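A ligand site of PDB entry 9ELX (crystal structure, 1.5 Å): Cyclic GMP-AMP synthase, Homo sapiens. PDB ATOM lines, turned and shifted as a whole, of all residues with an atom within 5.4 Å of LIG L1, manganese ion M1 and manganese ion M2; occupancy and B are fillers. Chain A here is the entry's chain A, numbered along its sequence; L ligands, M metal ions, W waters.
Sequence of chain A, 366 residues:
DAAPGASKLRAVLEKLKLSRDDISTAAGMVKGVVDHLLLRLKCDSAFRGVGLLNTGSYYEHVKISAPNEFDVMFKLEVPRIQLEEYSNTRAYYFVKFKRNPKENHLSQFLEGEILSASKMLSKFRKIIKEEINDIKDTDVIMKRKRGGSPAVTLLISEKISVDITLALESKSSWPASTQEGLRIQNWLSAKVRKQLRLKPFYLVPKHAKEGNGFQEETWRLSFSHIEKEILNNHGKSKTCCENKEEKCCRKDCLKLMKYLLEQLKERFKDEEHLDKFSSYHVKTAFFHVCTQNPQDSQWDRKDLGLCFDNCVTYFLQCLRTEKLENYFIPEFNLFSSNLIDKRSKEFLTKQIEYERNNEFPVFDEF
An oxygen (O3) of LIG L1 sits at hydrogen-bond distance from the guanidinium group of Arg 146 (2.8 Å).
The side-chain hydroxyl (OG) of Ser 149 lies within hydrogen-bond range of an oxygen (O3) of LIG L1 (2.9 Å).
An oxygen (O4) of LIG L1 lies within hydrogen-bond range of the side-chain amino group of Lys 206 (3.0 Å).
The guanidinium group (NH1) of Arg 220 sits at hydrogen-bond distance from a nitrogen (N5) of LG2 L2 (3.5 Å).
An oxygen (O5) of LG2 L2 lies close to the backbone NH (N) of Ser 57 (2.8 Å).
The side-chain hydroxyl (OG) of Ser 57 lies within hydrogen-bond range of an oxygen (O1) of LG2 L2 (2.6 Å).
OG of Ser 224 lies within hydrogen-bond range of O12 of LG2 L2 (2.9 Å).
NH2 of Arg 146 lies within salt-bridge range of OD1 of Asp 163.
The backbone NH (N) of Asp 163 is in hydrogen-bond range of the backbone carbonyl oxygen (O) of Phe 70.
The side-chain hydroxyl (OG) of Ser 149 is in hydrogen-bond range of the guanidinium group (NH1) of Arg 146 (3.4 Å).
OG of Ser 149 is in hydrogen-bond range of N of Ala 151 (3.0 Å).
O of Lys 206 sits close to N of Arg 220, at 3.5 Å.
O of Gly 148 is in hydrogen-bond range of NZ of Lys 206, at 2.9 Å.
The side-chain hydroxyl (OG) of Ser 222 is in hydrogen-bond range of the side-chain hydroxyl (OG) of Ser 224 (3.2 Å).
The backbone carbonyl oxygen of Val 204 lies within hydrogen-bond range of the backbone NH of Arg 220, 2.8 Å away.
A fluorine (F1) of LIG L1 lies close to the side-chain hydroxyl (OG) of Ser 222 (3.0 Å).
Merely in contact with LIG L1: Val 204, Arg 220, Pro 150, Gly 148 and Ser 224.
Hydrophobic or aromatic side chains within 4 Å of LIG L1: Pro 150 and Val 204.
12 residues have an atom within 4 Å of LIG L1: Glu 69, Asp 71, Arg 146, Gly 148, Ser 149, Pro 150, Asp 163, Val 204, Lys 206, Arg 220, Ser 222 and Ser 224.
The nearest printed residue that does not touch manganese ion M1 is Phe 70 (4.8 Å).
Merely in contact with manganese ion M2: Ser 57.
Manganese ion M1 is bound by OE2 of Glu 69 (2.1 Å), OD2 of Asp 163 (2.1 Å), OD1 of Asp 71 (2.1 Å), O1 of LIG L1 (2.2 Å), O7 of LG2 L2 (2.2 Å) and N3 of LIG L1 (2.3 Å).
Manganese ion M1 has six donor atoms within binding distance.
Manganese ion M2 is bound by OE1 of Glu 69 (2.1 Å), O3 of LG2 L2 (2.2 Å), O5 of LG2 L2 (2.2 Å), OD2 of Asp 71 (2.2 Å), O7 of LG2 L2 (2.2 Å) and water W2 (2.3 Å).
Manganese ion M2 has six donor atoms within binding distance.
Water W2 bridges OG of Ser 57 (2.7 Å) and O of Glu 69 (2.8 Å).
Water W3 lies within hydrogen-bond range of OG of Ser 222 (2.8 Å), SD of Met 73 (2.8 Å) and OG of Ser 224 (2.9 Å).
Water W4 lies within hydrogen-bond range of O6 of LG2 L2 (2.9 Å) and N1 of LIG L1 (2.9 Å).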
ATOM      1  N   GLY A  56      25.672  -6.263  -2.951  1.00  0.00           N
ATOM      2  CA  GLY A  56      25.581  -7.377  -3.902  1.00  0.00           C
ATOM      3  C   GLY A  56      24.939  -7.036  -5.236  1.00  0.00           C
ATOM      4  O   GLY A  56      24.557  -5.884  -5.487  1.00  0.00           O
ATOM      5  N   SER A  57      24.764  -8.068  -6.084  1.00  0.00           N
ATOM      6  CA  SER A  57      24.536  -7.789  -7.497  1.00  0.00           C
ATOM      7  C   SER A  57      23.190  -7.133  -7.776  1.00  0.00           C
ATOM      8  O   SER A  57      23.063  -6.390  -8.758  1.00  0.00           O
ATOM      9  CB  SER A  57      24.672  -9.049  -8.303  1.00  0.00           C
ATOM     10  OG  SER A  57      23.661 -10.011  -7.944  1.00  0.00           O
ATOM     11  N   GLU A  69      17.963 -13.529  -5.681  1.00  0.00           N
ATOM     12  CA  GLU A  69      19.030 -13.607  -4.681  1.00  0.00           C
ATOM     13  C   GLU A  69      19.479 -12.202  -4.335  1.00  0.00           C
ATOM     14  O   GLU A  69      19.940 -11.421  -5.195  1.00  0.00           O
ATOM     15  CB  GLU A  69      20.196 -14.462  -5.192  1.00  0.00           C
ATOM     16  CG  GLU A  69      21.044 -15.082  -4.015  1.00  0.00           C
ATOM     17  CD  GLU A  69      22.262 -14.249  -3.639  1.00  0.00           C
ATOM     18  OE1 GLU A  69      22.378 -13.105  -4.151  1.00  0.00           O
ATOM     19  OE2 GLU A  69      23.095 -14.747  -2.838  1.00  0.00           O
ATOM     20  N   PHE A  70      19.251 -11.850  -3.055  1.00  0.00           N
ATOM     21  CA  PHE A  70      19.493 -10.517  -2.543  1.00  0.00           C
ATOM     22  C   PHE A  70      20.481 -10.602  -1.400  1.00  0.00           C
ATOM     23  O   PHE A  70      20.440 -11.545  -0.631  1.00  0.00           O
ATOM     24  CB  PHE A  70      18.207  -9.875  -2.033  1.00  0.00           C
ATOM     25  CG  PHE A  70      17.200  -9.564  -3.100  1.00  0.00           C
ATOM     26  CD1 PHE A  70      16.460 -10.586  -3.686  1.00  0.00           C
ATOM     27  CD2 PHE A  70      16.940  -8.241  -3.455  1.00  0.00           C
ATOM     28  CE1 PHE A  70      15.510 -10.299  -4.623  1.00  0.00           C
ATOM     29  CE2 PHE A  70      15.933  -7.946  -4.398  1.00  0.00           C
ATOM     30  CZ  PHE A  70      15.256  -8.989  -5.007  1.00  0.00           C
ATOM     31  N   ASP A  71      21.283  -9.550  -1.244  1.00  0.00           N
ATOM     32  CA  ASP A  71      22.282  -9.494  -0.198  1.00  0.00           C
ATOM     33  C   ASP A  71      22.124  -8.216   0.592  1.00  0.00           C
ATOM     34  O   ASP A  71      21.914  -7.161   0.003  1.00  0.00           O
ATOM     35  CB  ASP A  71      23.686  -9.552  -0.789  1.00  0.00           C
ATOM     36  CG  ASP A  71      23.859 -10.756  -1.644  1.00  0.00           C
ATOM     37  OD1 ASP A  71      23.906 -11.892  -1.127  1.00  0.00           O
ATOM     38  OD2 ASP A  71      23.901 -10.587  -2.888  1.00  0.00           O
ATOM     39  N   MET A  73      23.399  -6.173   4.455  1.00  0.00           N
ATOM     40  CA  MET A  73      24.162  -6.193   5.690  1.00  0.00           C
ATOM     41  C   MET A  73      23.303  -5.561   6.773  1.00  0.00           C
ATOM     42  O   MET A  73      22.644  -4.532   6.542  1.00  0.00           O
ATOM     43  CB  MET A  73      25.457  -5.392   5.577  1.00  0.00           C
ATOM     44  CG  MET A  73      26.583  -6.224   5.013  1.00  0.00           C
ATOM     45  SD  MET A  73      28.210  -5.438   5.132  1.00  0.00           S
ATOM     46  CE  MET A  73      27.811  -3.908   5.932  1.00  0.00           C
ATOM     47  N   ARG A 146      25.663 -22.522   5.744  1.00  0.00           N
ATOM     48  CA  ARG A 146      26.665 -22.953   4.783  1.00  0.00           C
ATOM     49  C   ARG A 146      28.051 -22.603   5.337  1.00  0.00           C
ATOM     50  O   ARG A 146      28.280 -21.478   5.786  1.00  0.00           O
ATOM     51  CB  ARG A 146      26.436 -22.359   3.380  1.00  0.00           C
ATOM     52  CG  ARG A 146      26.944 -20.961   3.107  1.00  0.00           C
ATOM     53  CD  ARG A 146      26.922 -20.559   1.613  1.00  0.00           C
ATOM     54  NE  ARG A 146      25.619 -20.216   1.023  1.00  0.00           N
ATOM     55  CZ  ARG A 146      25.013 -19.038   1.125  1.00  0.00           C
ATOM     56  NH1 ARG A 146      25.514 -18.053   1.847  1.00  0.00           N
ATOM     57  NH2 ARG A 146      23.870 -18.831   0.452  1.00  0.00           N
ATOM     58  N   GLY A 148      31.750 -21.591   6.301  1.00  0.00           N
ATOM     59  CA  GLY A 148      32.564 -20.471   5.879  1.00  0.00           C
ATOM     60  C   GLY A 148      31.788 -19.206   5.559  1.00  0.00           C
ATOM     61  O   GLY A 148      32.406 -18.184   5.254  1.00  0.00           O
ATOM     62  N   SER A 149      30.453 -19.247   5.604  1.00  0.00           N
ATOM     63  CA  SER A 149      29.781 -18.006   5.219  1.00  0.00           C
ATOM     64  C   SER A 149      29.511 -17.135   6.420  1.00  0.00           C
ATOM     65  O   SER A 149      29.123 -17.640   7.478  1.00  0.00           O
ATOM     66  CB  SER A 149      28.450 -18.288   4.537  1.00  0.00           C
ATOM     67  OG  SER A 149      27.793 -17.085   4.155  1.00  0.00           O
ATOM     68  N   PRO A 150      29.622 -15.812   6.300  1.00  0.00           N
ATOM     69  CA  PRO A 150      29.206 -14.943   7.385  1.00  0.00           C
ATOM     70  C   PRO A 150      27.724 -14.631   7.347  1.00  0.00           C
ATOM     71  O   PRO A 150      27.277 -13.922   8.230  1.00  0.00           O
ATOM     72  CB  PRO A 150      30.027 -13.673   7.148  1.00  0.00           C
ATOM     73  CG  PRO A 150      30.072 -13.572   5.653  1.00  0.00           C
ATOM     74  CD  PRO A 150      30.154 -15.040   5.158  1.00  0.00           C
ATOM     75  N   ALA A 151      27.000 -15.108   6.315  1.00  0.00           N
ATOM     76  CA  ALA A 151      25.603 -14.733   6.147  1.00  0.00           C
ATOM     77  C   ALA A 151      24.690 -15.725   6.846  1.00  0.00           C
ATOM     78  O   ALA A 151      25.022 -16.915   7.018  1.00  0.00           O
ATOM     79  CB  ALA A 151      25.249 -14.675   4.648  1.00  0.00           C
ATOM     80  N   ASP A 163      20.579 -13.200   1.700  1.00  0.00           N
ATOM     81  CA  ASP A 163      21.720 -13.394   2.591  1.00  0.00           C
ATOM     82  C   ASP A 163      21.818 -12.176   3.464  1.00  0.00           C
ATOM     83  O   ASP A 163      21.993 -11.067   2.938  1.00  0.00           O
ATOM     84  CB  ASP A 163      23.024 -13.561   1.800  1.00  0.00           C
ATOM     85  CG  ASP A 163      23.079 -14.839   1.085  1.00  0.00           C
ATOM     86  OD1 ASP A 163      22.988 -15.926   1.668  1.00  0.00           O
ATOM     87  OD2 ASP A 163      23.430 -14.834  -0.105  1.00  0.00           O
ATOM     88  N   THR A 165      24.002 -10.436   6.344  1.00  0.00           N
ATOM     89  CA  THR A 165      25.313 -10.540   6.976  1.00  0.00           C
ATOM     90  C   THR A 165      25.405  -9.531   8.100  1.00  0.00           C
ATOM     91  O   THR A 165      25.260  -8.325   7.880  1.00  0.00           O
ATOM     92  CB  THR A 165      26.427 -10.323   5.955  1.00  0.00           C
ATOM     93  OG1 THR A 165      26.397 -11.371   4.982  1.00  0.00           O
ATOM     94  CG2 THR A 165      27.824 -10.297   6.616  1.00  0.00           C
ATOM     95  N   VAL A 204      32.892  -8.521   9.176  1.00  0.00           N
ATOM     96  CA  VAL A 204      31.831  -9.519   9.122  1.00  0.00           C
ATOM     97  C   VAL A 204      32.372 -10.817   9.727  1.00  0.00           C
ATOM     98  O   VAL A 204      33.600 -11.053   9.757  1.00  0.00           O
ATOM     99  CB  VAL A 204      31.305  -9.714   7.679  1.00  0.00           C
ATOM    100  CG1 VAL A 204      30.780  -8.394   7.132  1.00  0.00           C
ATOM    101  CG2 VAL A 204      32.449 -10.253   6.787  1.00  0.00           C
ATOM    102  N   LYS A 206      33.240 -13.802   9.161  1.00  0.00           N
ATOM    103  CA  LYS A 206      33.899 -14.829   8.361  1.00  0.00           C
ATOM    104  C   LYS A 206      35.268 -15.032   8.975  1.00  0.00           C
ATOM    105  O   LYS A 206      36.035 -14.069   9.128  1.00  0.00           O
ATOM    106  CB  LYS A 206      33.994 -14.386   6.892  1.00  0.00           C
ATOM    107  CG  LYS A 206      34.594 -15.463   5.989  1.00  0.00           C
ATOM    108  CD  LYS A 206      34.823 -14.908   4.604  1.00  0.00           C
ATOM    109  CE  LYS A 206      35.396 -15.954   3.632  1.00  0.00           C
ATOM    110  NZ  LYS A 206      34.579 -17.175   3.569  1.00  0.00           N
ATOM    111  N   ARG A 220      36.319 -10.610   9.319  1.00  0.00           N
ATOM    112  CA  ARG A 220      36.873 -10.343   7.999  1.00  0.00           C
ATOM    113  C   ARG A 220      36.519  -8.925   7.579  1.00  0.00           C
ATOM    114  O   ARG A 220      35.381  -8.491   7.728  1.00  0.00           O
ATOM    115  CB  ARG A 220      36.327 -11.352   6.981  1.00  0.00           C
ATOM    116  CG  ARG A 220      36.445 -10.858   5.562  1.00  0.00           C
ATOM    117  CD  ARG A 220      37.856 -11.022   5.043  1.00  0.00           C
ATOM    118  NE  ARG A 220      37.962 -12.321   4.425  1.00  0.00           N
ATOM    119  CZ  ARG A 220      37.784 -12.548   3.124  1.00  0.00           C
ATOM    120  NH1 ARG A 220      37.428 -11.580   2.302  1.00  0.00           N
ATOM    121  NH2 ARG A 220      37.916 -13.798   2.672  1.00  0.00           N
ATOM    122  N   LEU A 221      37.499  -8.191   7.057  1.00  0.00           N
ATOM    123  CA  LEU A 221      37.237  -6.867   6.504  1.00  0.00           C
ATOM    124  C   LEU A 221      36.314  -6.958   5.302  1.00  0.00           C
ATOM    125  O   LEU A 221      36.476  -7.846   4.443  1.00  0.00           O
ATOM    126  CB  LEU A 221      38.544  -6.235   6.033  1.00  0.00           C
ATOM    127  CG  LEU A 221      39.490  -5.707   7.069  1.00  0.00           C
ATOM    128  CD1 LEU A 221      40.658  -5.084   6.276  1.00  0.00           C
ATOM    129  CD2 LEU A 221      38.785  -4.659   7.961  1.00  0.00           C
ATOM    130  N   SER A 222      35.379  -6.032   5.204  1.00  0.00           N
ATOM    131  CA  SER A 222      34.457  -5.993   4.090  1.00  0.00           C
ATOM    132  C   SER A 222      34.273  -4.571   3.626  1.00  0.00           C
ATOM    133  O   SER A 222      34.011  -3.644   4.415  1.00  0.00           O
ATOM    134  CB  SER A 222      33.080  -6.586   4.438  1.00  0.00           C
ATOM    135  OG  SER A 222      32.220  -6.445   3.293  1.00  0.00           O
ATOM    136  N   SER A 224      31.986  -4.141   0.852  1.00  0.00           N
ATOM    137  CA  SER A 224      30.897  -4.371  -0.101  1.00  0.00           C
ATOM    138  C   SER A 224      30.219  -3.043  -0.474  1.00  0.00           C
ATOM    139  O   SER A 224      29.797  -2.858  -1.624  1.00  0.00           O
ATOM    140  CB  SER A 224      29.841  -5.322   0.495  1.00  0.00           C
ATOM    141  OG  SER A 224      30.330  -6.629   0.709  1.00  0.00           O
HETATM  142  C1  LIG L   1      31.274 -15.614   1.682  1.00  0.00           C
HETATM  143  N1  LIG L   1      29.845 -16.789   0.055  1.00  0.00           N
HETATM  144  C2  LIG L   1      28.533 -17.091   0.222  1.00  0.00           C
HETATM  145  C3  LIG L   1      27.314 -18.007  -1.710  1.00  0.00           C
HETATM  146  C4  LIG L   1      25.600 -16.721  -2.764  1.00  0.00           C
HETATM  147  C5  LIG L   1      26.942 -14.529  -0.012  1.00  0.00           C
HETATM  148  C6  LIG L   1      31.016 -10.589   3.028  1.00  0.00           C
HETATM  149  C7  LIG L   1      29.742 -10.986   2.734  1.00  0.00           C
HETATM  150  C8  LIG L   1      29.628 -12.272   2.240  1.00  0.00           C
HETATM  151  C9  LIG L   1      30.718 -13.148   2.061  1.00  0.00           C
HETATM  152  C10 LIG L   1      31.989 -12.711   2.387  1.00  0.00           C
HETATM  153  C11 LIG L   1      32.096 -11.403   2.890  1.00  0.00           C
HETATM  154  C12 LIG L   1      30.847 -16.933   1.095  1.00  0.00           C
HETATM  155  C13 LIG L   1      27.563 -16.965  -0.830  1.00  0.00           C
HETATM  156  C14 LIG L   1      26.320 -17.924  -2.708  1.00  0.00           C
HETATM  157  C15 LIG L   1      26.752 -15.811  -0.935  1.00  0.00           C
HETATM  158  F1  LIG L   1      31.192  -9.305   3.540  1.00  0.00           F
HETATM  159  N2  LIG L   1      30.476 -14.454   1.560  1.00  0.00           N
HETATM  160  N3  LIG L   1      25.812 -15.740  -1.866  1.00  0.00           N
HETATM  161  O1  LIG L   1      26.120 -13.642  -0.161  1.00  0.00           O
HETATM  162  O2  LIG L   1      27.945 -14.529   0.710  1.00  0.00           O
HETATM  163  O3  LIG L   1      28.199 -17.472   1.342  1.00  0.00           O
HETATM  164  O4  LIG L   1      32.353 -15.566   2.293  1.00  0.00           O
HETATM  165 CL1  LIG L   1      33.650 -10.798   3.273  1.00  0.00          CL
HETATM  166  P1  LG2 L   2      25.404 -13.019  -7.535  1.00  0.00           P
HETATM  167  O1  LG2 L   2      24.770 -12.248  -8.602  1.00  0.00           O
HETATM  168  O2  LG2 L   2      25.868 -14.422  -8.030  1.00  0.00           O
HETATM  169  O3  LG2 L   2      24.526 -13.130  -6.326  1.00  0.00           O
HETATM  170  P2  LG2 L   2      26.973 -11.167  -5.843  1.00  0.00           P
HETATM  171  O4  LG2 L   2      28.009 -10.154  -6.161  1.00  0.00           O
HETATM  172  O5  LG2 L   2      25.656 -10.603  -5.293  1.00  0.00           O
HETATM  173  N1  LG2 L   2      26.795 -12.150  -7.170  1.00  0.00           N
HETATM  174  P3  LG2 L   2      27.184 -12.852  -3.419  1.00  0.00           P
HETATM  175  O6  LG2 L   2      27.955 -14.133  -3.372  1.00  0.00           O
HETATM  176  O7  LG2 L   2      25.667 -12.944  -3.336  1.00  0.00           O
HETATM  177  O8  LG2 L   2      27.630 -12.064  -4.742  1.00  0.00           O
HETATM  178  O9  LG2 L   2      27.757 -11.910  -2.322  1.00  0.00           O
HETATM  179  C1  LG2 L   2      27.143 -10.632  -2.115  1.00  0.00           C
HETATM  180  C2  LG2 L   2      28.251  -9.614  -1.932  1.00  0.00           C
HETATM  181  O10 LG2 L   2      29.000  -9.993  -0.755  1.00  0.00           O
HETATM  182  C3  LG2 L   2      29.298  -9.533  -3.019  1.00  0.00           C
HETATM  183  O11 LG2 L   2      28.922  -8.660  -4.080  1.00  0.00           O
HETATM  184  C4  LG2 L   2      30.491  -8.952  -2.274  1.00  0.00           C
HETATM  185  O12 LG2 L   2      30.311  -7.549  -2.091  1.00  0.00           O
HETATM  186  C5  LG2 L   2      30.372  -9.661  -0.936  1.00  0.00           C
HETATM  187  N2  LG2 L   2      31.163 -10.898  -0.933  1.00  0.00           N
HETATM  188  C6  LG2 L   2      30.772 -12.147  -1.351  1.00  0.00           C
HETATM  189  N3  LG2 L   2      31.736 -13.042  -1.338  1.00  0.00           N
HETATM  190  C7  LG2 L   2      32.828 -12.335  -0.868  1.00  0.00           C
HETATM  191  C8  LG2 L   2      34.164 -12.702  -0.613  1.00  0.00           C
HETATM  192  N4  LG2 L   2      34.624 -13.949  -0.782  1.00  0.00           N
HETATM  193  N5  LG2 L   2      35.002 -11.738  -0.189  1.00  0.00           N
HETATM  194  C9  LG2 L   2      34.532 -10.506   0.007  1.00  0.00           C
HETATM  195  N6  LG2 L   2      33.295 -10.034  -0.205  1.00  0.00           N
HETATM  196  C10 LG2 L   2      32.496 -11.009  -0.639  1.00  0.00           C
HETATM  197 MN    MN M   1      24.556 -13.861  -1.628  1.00  0.00          MN
HETATM  198 MN    MN M   2      24.125 -11.954  -4.568  1.00  0.00          MN
HETATM  199  O   HOH W   1      26.661 -11.282   1.152  1.00  0.00           O
HETATM  200  O   HOH W   2      22.584 -10.649  -5.592  1.00  0.00           O
HETATM  201  O   HOH W   3      29.531  -7.276   3.403  1.00  0.00           O
HETATM  202  O   HOH W   4      30.382 -15.352  -2.409  1.00  0.00           O
